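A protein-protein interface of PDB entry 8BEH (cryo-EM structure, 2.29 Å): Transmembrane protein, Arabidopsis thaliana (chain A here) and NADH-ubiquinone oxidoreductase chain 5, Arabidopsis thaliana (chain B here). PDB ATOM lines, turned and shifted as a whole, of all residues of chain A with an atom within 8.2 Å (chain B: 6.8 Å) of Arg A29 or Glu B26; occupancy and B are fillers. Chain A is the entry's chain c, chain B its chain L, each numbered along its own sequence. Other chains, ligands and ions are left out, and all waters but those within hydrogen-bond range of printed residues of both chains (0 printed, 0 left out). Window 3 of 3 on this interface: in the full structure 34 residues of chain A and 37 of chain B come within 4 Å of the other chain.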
ATOM      1  N   THR A  23     -13.137  22.519  16.526  1.00  0.00           N
ATOM      2  CA  THR A  23     -13.581  23.245  15.343  1.00  0.00           C
ATOM      3  C   THR A  23     -14.828  22.630  14.721  1.00  0.00           C
ATOM      4  O   THR A  23     -15.425  23.242  13.830  1.00  0.00           O
ATOM      5  CB  THR A  23     -12.440  23.312  14.324  1.00  0.00           C
ATOM      6  OG1 THR A  23     -11.205  23.530  15.015  1.00  0.00           O
ATOM      7  CG2 THR A  23     -12.640  24.468  13.356  1.00  0.00           C
ATOM      8  N   GLY A  24     -15.242  21.449  15.177  1.00  0.00           N
ATOM      9  CA  GLY A  24     -16.511  20.875  14.795  1.00  0.00           C
ATOM     10  C   GLY A  24     -16.459  19.761  13.772  1.00  0.00           C
ATOM     11  O   GLY A  24     -17.486  19.120  13.542  1.00  0.00           O
ATOM     12  N   GLY A  25     -15.315  19.513  13.145  1.00  0.00           N
ATOM     13  CA  GLY A  25     -15.211  18.454  12.168  1.00  0.00           C
ATOM     14  C   GLY A  25     -15.877  18.791  10.847  1.00  0.00           C
ATOM     15  O   GLY A  25     -16.250  19.936  10.590  1.00  0.00           O
ATOM     16  N   PRO A  26     -16.050  17.790   9.987  1.00  0.00           N
ATOM     17  CA  PRO A  26     -16.542  18.051   8.629  1.00  0.00           C
ATOM     18  C   PRO A  26     -18.038  18.330   8.569  1.00  0.00           C
ATOM     19  O   PRO A  26     -18.846  17.640   9.193  1.00  0.00           O
ATOM     20  CB  PRO A  26     -16.196  16.757   7.882  1.00  0.00           C
ATOM     21  CG  PRO A  26     -16.209  15.710   8.942  1.00  0.00           C
ATOM     22  CD  PRO A  26     -15.731  16.367  10.200  1.00  0.00           C
ATOM     23  N   ASN A  27     -18.394  19.348   7.780  1.00  0.00           N
ATOM     24  CA  ASN A  27     -19.790  19.693   7.488  1.00  0.00           C
ATOM     25  C   ASN A  27     -20.577  19.976   8.766  1.00  0.00           C
ATOM     26  O   ASN A  27     -21.661  19.439   8.985  1.00  0.00           O
ATOM     27  CB  ASN A  27     -20.462  18.594   6.662  1.00  0.00           C
ATOM     28  CG  ASN A  27     -19.816  18.403   5.307  1.00  0.00           C
ATOM     29  OD1 ASN A  27     -19.717  19.336   4.518  1.00  0.00           O
ATOM     30  ND2 ASN A  27     -19.346  17.194   5.043  1.00  0.00           N
ATOM     31  N   CYS A  28     -20.017  20.831   9.616  1.00  0.00           N
ATOM     32  CA  CYS A  28     -20.609  21.118  10.917  1.00  0.00           C
ATOM     33  C   CYS A  28     -21.780  22.088  10.760  1.00  0.00           C
ATOM     34  O   CYS A  28     -21.604  23.216  10.289  1.00  0.00           O
ATOM     35  CB  CYS A  28     -19.551  21.683  11.861  1.00  0.00           C
ATOM     36  SG  CYS A  28     -20.118  21.955  13.548  1.00  0.00           S
ATOM     37  N   ARG A  29     -22.967  21.643  11.166  1.00  0.00           N
ATOM     38  CA  ARG A  29     -24.211  22.408  11.047  1.00  0.00           C
ATOM     39  C   ARG A  29     -24.956  22.385  12.374  1.00  0.00           C
ATOM     40  O   ARG A  29     -26.006  21.745  12.489  1.00  0.00           O
ATOM     41  CB  ARG A  29     -25.102  21.810   9.958  1.00  0.00           C
ATOM     42  CG  ARG A  29     -24.531  21.821   8.560  1.00  0.00           C
ATOM     43  CD  ARG A  29     -24.672  23.174   7.910  1.00  0.00           C
ATOM     44  NE  ARG A  29     -26.057  23.617   7.996  1.00  0.00           N
ATOM     45  CZ  ARG A  29     -26.518  24.754   7.501  1.00  0.00           C
ATOM     46  NH1 ARG A  29     -25.775  25.516   6.720  1.00  0.00           N
ATOM     47  NH2 ARG A  29     -27.772  25.113   7.757  1.00  0.00           N
ATOM     48  N   PRO A  30     -24.449  23.070  13.400  1.00  0.00           N
ATOM     49  CA  PRO A  30     -25.167  23.093  14.682  1.00  0.00           C
ATOM     50  C   PRO A  30     -26.553  23.705  14.528  1.00  0.00           C
ATOM     51  O   PRO A  30     -26.751  24.667  13.782  1.00  0.00           O
ATOM     52  CB  PRO A  30     -24.263  23.940  15.586  1.00  0.00           C
ATOM     53  CG  PRO A  30     -23.365  24.673  14.666  1.00  0.00           C
ATOM     54  CD  PRO A  30     -23.193  23.831  13.457  1.00  0.00           C
ATOM     55  N   LYS A  31     -27.519  23.128  15.247  1.00  0.00           N
ATOM     56  CA  LYS A  31     -28.914  23.518  15.074  1.00  0.00           C
ATOM     57  C   LYS A  31     -29.155  24.956  15.515  1.00  0.00           C
ATOM     58  O   LYS A  31     -29.916  25.690  14.875  1.00  0.00           O
ATOM     59  CB  LYS A  31     -29.826  22.558  15.840  1.00  0.00           C
ATOM     60  CG  LYS A  31     -31.212  23.097  16.110  1.00  0.00           C
ATOM     61  CD  LYS A  31     -31.773  22.549  17.408  1.00  0.00           C
ATOM     62  CE  LYS A  31     -33.038  21.739  17.165  1.00  0.00           C
ATOM     63  NZ  LYS A  31     -33.865  21.599  18.396  1.00  0.00           N
ATOM     64  N   HIS A  32     -28.507  25.380  16.594  1.00  0.00           N
ATOM     65  CA  HIS A  32     -28.691  26.717  17.152  1.00  0.00           C
ATOM     66  C   HIS A  32     -27.555  27.654  16.777  1.00  0.00           C
ATOM     67  O   HIS A  32     -27.157  28.504  17.575  1.00  0.00           O
ATOM     68  CB  HIS A  32     -28.840  26.631  18.664  1.00  0.00           C
ATOM     69  CG  HIS A  32     -30.066  25.897  19.102  1.00  0.00           C
ATOM     70  ND1 HIS A  32     -31.330  26.255  18.688  1.00  0.00           N
ATOM     71  CD2 HIS A  32     -30.222  24.821  19.907  1.00  0.00           C
ATOM     72  CE1 HIS A  32     -32.213  25.434  19.227  1.00  0.00           C
ATOM     73  NE2 HIS A  32     -31.567  24.557  19.973  1.00  0.00           N
ATOM     74  N   TRP A  33     -27.028  27.528  15.558  1.00  0.00           N
ATOM     75  CA  TRP A  33     -25.816  28.258  15.205  1.00  0.00           C
ATOM     76  C   TRP A  33     -26.039  29.767  15.151  1.00  0.00           C
ATOM     77  O   TRP A  33     -25.098  30.526  15.384  1.00  0.00           O
ATOM     78  CB  TRP A  33     -25.253  27.747  13.877  1.00  0.00           C
ATOM     79  CG  TRP A  33     -26.042  28.134  12.673  1.00  0.00           C
ATOM     80  CD1 TRP A  33     -27.010  27.403  12.058  1.00  0.00           C
ATOM     81  CD2 TRP A  33     -25.922  29.350  11.925  1.00  0.00           C
ATOM     82  NE1 TRP A  33     -27.504  28.085  10.978  1.00  0.00           N
ATOM     83  CE2 TRP A  33     -26.853  29.284  10.872  1.00  0.00           C
ATOM     84  CE3 TRP A  33     -25.118  30.486  12.045  1.00  0.00           C
ATOM     85  CZ2 TRP A  33     -27.006  30.312   9.946  1.00  0.00           C
ATOM     86  CZ3 TRP A  33     -25.269  31.504  11.124  1.00  0.00           C
ATOM     87  CH2 TRP A  33     -26.205  31.411  10.089  1.00  0.00           C
ATOM     88  N   ARG A  34     -27.259  30.223  14.853  1.00  0.00           N
ATOM     89  CA  ARG A  34     -27.523  31.662  14.834  1.00  0.00           C
ATOM     90  C   ARG A  34     -27.434  32.270  16.227  1.00  0.00           C
ATOM     91  O   ARG A  34     -26.757  33.286  16.430  1.00  0.00           O
ATOM     92  CB  ARG A  34     -28.890  31.952  14.223  1.00  0.00           C
ATOM     93  CG  ARG A  34     -28.875  32.002  12.724  1.00  0.00           C
ATOM     94  CD  ARG A  34     -30.207  31.640  12.151  1.00  0.00           C
ATOM     95  NE  ARG A  34     -30.027  30.693  11.066  1.00  0.00           N
ATOM     96  CZ  ARG A  34     -30.911  29.772  10.718  1.00  0.00           C
ATOM     97  NH1 ARG A  34     -32.077  29.664  11.335  1.00  0.00           N
ATOM     98  NH2 ARG A  34     -30.615  28.939   9.728  1.00  0.00           N
ATOM     99  N   THR A  37     -23.923  32.242  17.342  1.00  0.00           N
ATOM    100  CA  THR A  37     -23.147  33.275  16.641  1.00  0.00           C
ATOM    101  C   THR A  37     -23.381  34.622  17.331  1.00  0.00           C
ATOM    102  O   THR A  37     -22.412  35.277  17.608  1.00  0.00           O
ATOM    103  CB  THR A  37     -23.367  33.195  15.127  1.00  0.00           C
ATOM    104  OG1 THR A  37     -22.905  31.924  14.694  1.00  0.00           O
ATOM    105  CG2 THR A  37     -22.623  34.276  14.374  1.00  0.00           C
ATOM    106  N   ARG B  21     -17.292  24.365  16.771  1.00  0.00           N
ATOM    107  CA  ARG B  21     -18.320  23.336  16.859  1.00  0.00           C
ATOM    108  C   ARG B  21     -19.685  23.907  17.231  1.00  0.00           C
ATOM    109  O   ARG B  21     -20.700  23.254  16.983  1.00  0.00           O
ATOM    110  CB  ARG B  21     -17.906  22.265  17.872  1.00  0.00           C
ATOM    111  CG  ARG B  21     -17.822  22.775  19.295  1.00  0.00           C
ATOM    112  CD  ARG B  21     -17.371  21.696  20.263  1.00  0.00           C
ATOM    113  NE  ARG B  21     -17.218  22.207  21.619  1.00  0.00           N
ATOM    114  CZ  ARG B  21     -16.173  22.899  22.051  1.00  0.00           C
ATOM    115  NH1 ARG B  21     -15.181  23.226  21.241  1.00  0.00           N
ATOM    116  NH2 ARG B  21     -16.122  23.272  23.326  1.00  0.00           N
ATOM    117  N   LEU B  23     -20.659  27.127  16.185  1.00  0.00           N
ATOM    118  CA  LEU B  23     -20.971  28.110  15.118  1.00  0.00           C
ATOM    119  C   LEU B  23     -21.145  27.449  13.779  1.00  0.00           C
ATOM    120  O   LEU B  23     -21.914  27.988  13.014  1.00  0.00           O
ATOM    121  CB  LEU B  23     -19.840  29.129  15.027  1.00  0.00           C
ATOM    122  CG  LEU B  23     -19.992  30.385  15.888  1.00  0.00           C
ATOM    123  CD1 LEU B  23     -20.207  30.080  17.358  1.00  0.00           C
ATOM    124  CD2 LEU B  23     -18.804  31.306  15.709  1.00  0.00           C
ATOM    125  N   GLY B  24     -20.476  26.324  13.546  1.00  0.00           N
ATOM    126  CA  GLY B  24     -20.466  25.736  12.240  1.00  0.00           C
ATOM    127  C   GLY B  24     -19.862  26.643  11.180  1.00  0.00           C
ATOM    128  O   GLY B  24     -19.263  27.685  11.447  1.00  0.00           O
ATOM    129  N   SER B  25     -20.058  26.204   9.940  1.00  0.00           N
ATOM    130  CA  SER B  25     -19.502  26.919   8.798  1.00  0.00           C
ATOM    131  C   SER B  25     -19.989  28.359   8.766  1.00  0.00           C
ATOM    132  O   SER B  25     -19.189  29.301   8.690  1.00  0.00           O
ATOM    133  CB  SER B  25     -19.886  26.202   7.507  1.00  0.00           C
ATOM    134  OG  SER B  25     -19.533  24.840   7.561  1.00  0.00           O
ATOM    135  N   GLU B  26     -21.307  28.544   8.858  1.00  0.00           N
ATOM    136  CA  GLU B  26     -21.898  29.867   8.704  1.00  0.00           C
ATOM    137  C   GLU B  26     -21.455  30.811   9.808  1.00  0.00           C
ATOM    138  O   GLU B  26     -21.003  31.932   9.532  1.00  0.00           O
ATOM    139  CB  GLU B  26     -23.418  29.750   8.673  1.00  0.00           C
ATOM    140  CG  GLU B  26     -23.947  29.328   7.335  1.00  0.00           C
ATOM    141  CD  GLU B  26     -23.914  27.845   7.152  1.00  0.00           C
ATOM    142  OE1 GLU B  26     -24.663  27.148   7.861  1.00  0.00           O
ATOM    143  OE2 GLU B  26     -23.125  27.377   6.307  1.00  0.00           O
ATOM    144  N   GLY B  27     -21.631  30.415  11.059  1.00  0.00           N
ATOM    145  CA  GLY B  27     -21.183  31.243  12.183  1.00  0.00           C
ATOM    146  C   GLY B  27     -19.741  31.654  12.108  1.00  0.00           C
ATOM    147  O   GLY B  27     -19.495  32.835  12.281  1.00  0.00           O
ATOM    148  N   SER B  28     -18.840  30.722  11.826  1.00  0.00           N
ATOM    149  CA  SER B  28     -17.387  30.925  11.783  1.00  0.00           C
ATOM    150  C   SER B  28     -17.025  31.851  10.603  1.00  0.00           C
ATOM    151  O   SER B  28     -16.212  32.737  10.817  1.00  0.00           O
ATOM    152  CB  SER B  28     -16.636  29.572  11.830  1.00  0.00           C
ATOM    153  OG  SER B  28     -16.904  28.835  13.006  1.00  0.00           O
ATOM    154  N   ALA B  29     -17.753  31.746   9.507  1.00  0.00           N
ATOM    155  CA  ALA B  29     -17.556  32.608   8.323  1.00  0.00           C
ATOM    156  C   ALA B  29     -17.878  34.069   8.714  1.00  0.00           C
ATOM    157  O   ALA B  29     -16.982  34.870   8.602  1.00  0.00           O
ATOM    158  CB  ALA B  29     -18.347  32.072   7.192  1.00  0.00           C
ATOM    159  N   ILE B  30     -18.990  34.262   9.383  1.00  0.00           N
ATOM    160  CA  ILE B  30     -19.467  35.567   9.871  1.00  0.00           C
ATOM    161  C   ILE B  30     -18.554  36.116  10.950  1.00  0.00           C
ATOM    162  O   ILE B  30     -18.127  37.239  10.799  1.00  0.00           O
ATOM    163  CB  ILE B  30     -20.923  35.427  10.365  1.00  0.00           C
ATOM    164  CG1 ILE B  30     -21.871  35.126   9.201  1.00  0.00           C
ATOM    165  CG2 ILE B  30     -21.358  36.658  11.135  1.00  0.00           C
ATOM    166  CD1 ILE B  30     -23.329  35.091   9.566  1.00  0.00           C
ATOM    167  N   MET B  31     -18.249  35.310  11.946  1.00  0.00           N
ATOM    168  CA  MET B  31     -17.491  35.788  13.090  1.00  0.00           C
ATOM    169  C   MET B  31     -16.149  36.308  12.592  1.00  0.00           C
ATOM    170  O   MET B  31     -15.781  37.421  13.027  1.00  0.00           O
ATOM    171  CB  MET B  31     -17.273  34.660  14.105  1.00  0.00           C
ATOM    172  CG  MET B  31     -17.297  35.081  15.519  1.00  0.00           C
ATOM    173  SD  MET B  31     -18.787  35.982  15.936  1.00  0.00           S
ATOM    174  CE  MET B  31     -17.958  37.277  16.853  1.00  0.00           C
ATOM    175  N   ILE B 101     -15.919  32.906   2.040  1.00  0.00           N
ATOM    176  CA  ILE B 101     -17.255  32.524   2.502  1.00  0.00           C
ATOM    177  C   ILE B 101     -18.002  31.740   1.429  1.00  0.00           C
ATOM    178  O   ILE B 101     -18.680  30.748   1.721  1.00  0.00           O
ATOM    179  CB  ILE B 101     -18.047  33.769   2.944  1.00  0.00           C
ATOM    180  CG1 ILE B 101     -17.601  34.217   4.333  1.00  0.00           C
ATOM    181  CG2 ILE B 101     -19.543  33.492   2.928  1.00  0.00           C
ATOM    182  CD1 ILE B 101     -18.324  35.438   4.839  1.00  0.00           C
ATOM    183  N   SER B 105     -17.503  27.164   0.325  1.00  0.00           N
ATOM    184  CA  SER B 105     -18.823  26.848   0.860  1.00  0.00           C
ATOM    185  C   SER B 105     -19.115  25.355   0.824  1.00  0.00           C
ATOM    186  O   SER B 105     -19.837  24.847   1.687  1.00  0.00           O
ATOM    187  CB  SER B 105     -19.893  27.620   0.091  1.00  0.00           C
ATOM    188  OG  SER B 105     -20.183  26.993  -1.141  1.00  0.00           O
ATOM    189  N   SER B 110     -14.521  24.331   6.481  1.00  0.00           N
ATOM    190  CA  SER B 110     -14.410  25.786   6.373  1.00  0.00           C
ATOM    191  C   SER B 110     -14.099  26.506   7.689  1.00  0.00           C
ATOM    192  O   SER B 110     -13.352  27.498   7.641  1.00  0.00           O
ATOM    193  CB  SER B 110     -15.676  26.353   5.713  1.00  0.00           C
ATOM    194  OG  SER B 110     -16.794  26.323   6.574  1.00  0.00           O
ATOM    195  N   PRO B 111     -14.640  26.121   8.859  1.00  0.00           N
ATOM    196  CA  PRO B 111     -14.281  26.863  10.084  1.00  0.00           C
ATOM    197  C   PRO B 111     -12.791  26.865  10.401  1.00  0.00           C
ATOM    198  O   PRO B 111     -12.247  27.911  10.783  1.00  0.00           O
ATOM    199  CB  PRO B 111     -15.097  26.149  11.172  1.00  0.00           C
ATOM    200  CG  PRO B 111     -16.217  25.525  10.447  1.00  0.00           C
ATOM    201  CD  PRO B 111     -15.652  25.088   9.146  1.00  0.00           C
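Thr A23 touches Arg B21 (C to N, 3.6 Å). Pro B111 touches Thr A23 (CB to CG2, 3.7 Å). Gly A24 touches Arg B21 (CA to CB, 3.7 Å). Gly B24 touches Cys A28 (CA to O, 3.4 Å). CG of Pro A30 touches C of Leu B23, 3.7 Å away. Pro A30 touches Gly B24 (CG to N, 3.5 Å). CB of Trp A33 touches O of Leu B23 (3.5 Å). Trp A33 touches Gly B27. Thr A37 touches Leu B23. Gly B27 touches Thr A37 (CA to OG1, 3.1 Å).
The backbone carbonyl oxygen of Trp A33 lies within hydrogen-bond range of the side-chain hydroxyl of Thr A37 (2.7 Å). The side-chain hydroxyl of Ser B28 sits at hydrogen-bond distance from the backbone carbonyl oxygen of Gly B24. OG of Ser B110 lies close to OG of Ser B25, at 3.3 Å.
Among the printed residues, 15 pairs touch across the chains.
OE2 of Glu B26 is in salt-bridge range of NH1 of Arg A29 (3.3 Å). O of Arg B21 sits at hydrogen-bond distance from SG of Cys A28. The backbone carbonyl oxygen of Cys A28 sits at hydrogen-bond distance from the backbone NH of Ser B25 (3.4 Å).
Of the printed residues of chain B, Gly A24 touches Arg B21 (3.7 Å). Printed residues of chain B within 4 Å of Arg A29: Glu B26. Of the printed residues of chain A, Gly B24 touches Cys A28 and Pro A30. Glu B26 touches just these residues of chain A: Arg A29 and Trp A33. The nearest residue of chain B that does not touch Arg A29 is Gly B24 (4.9 Å).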
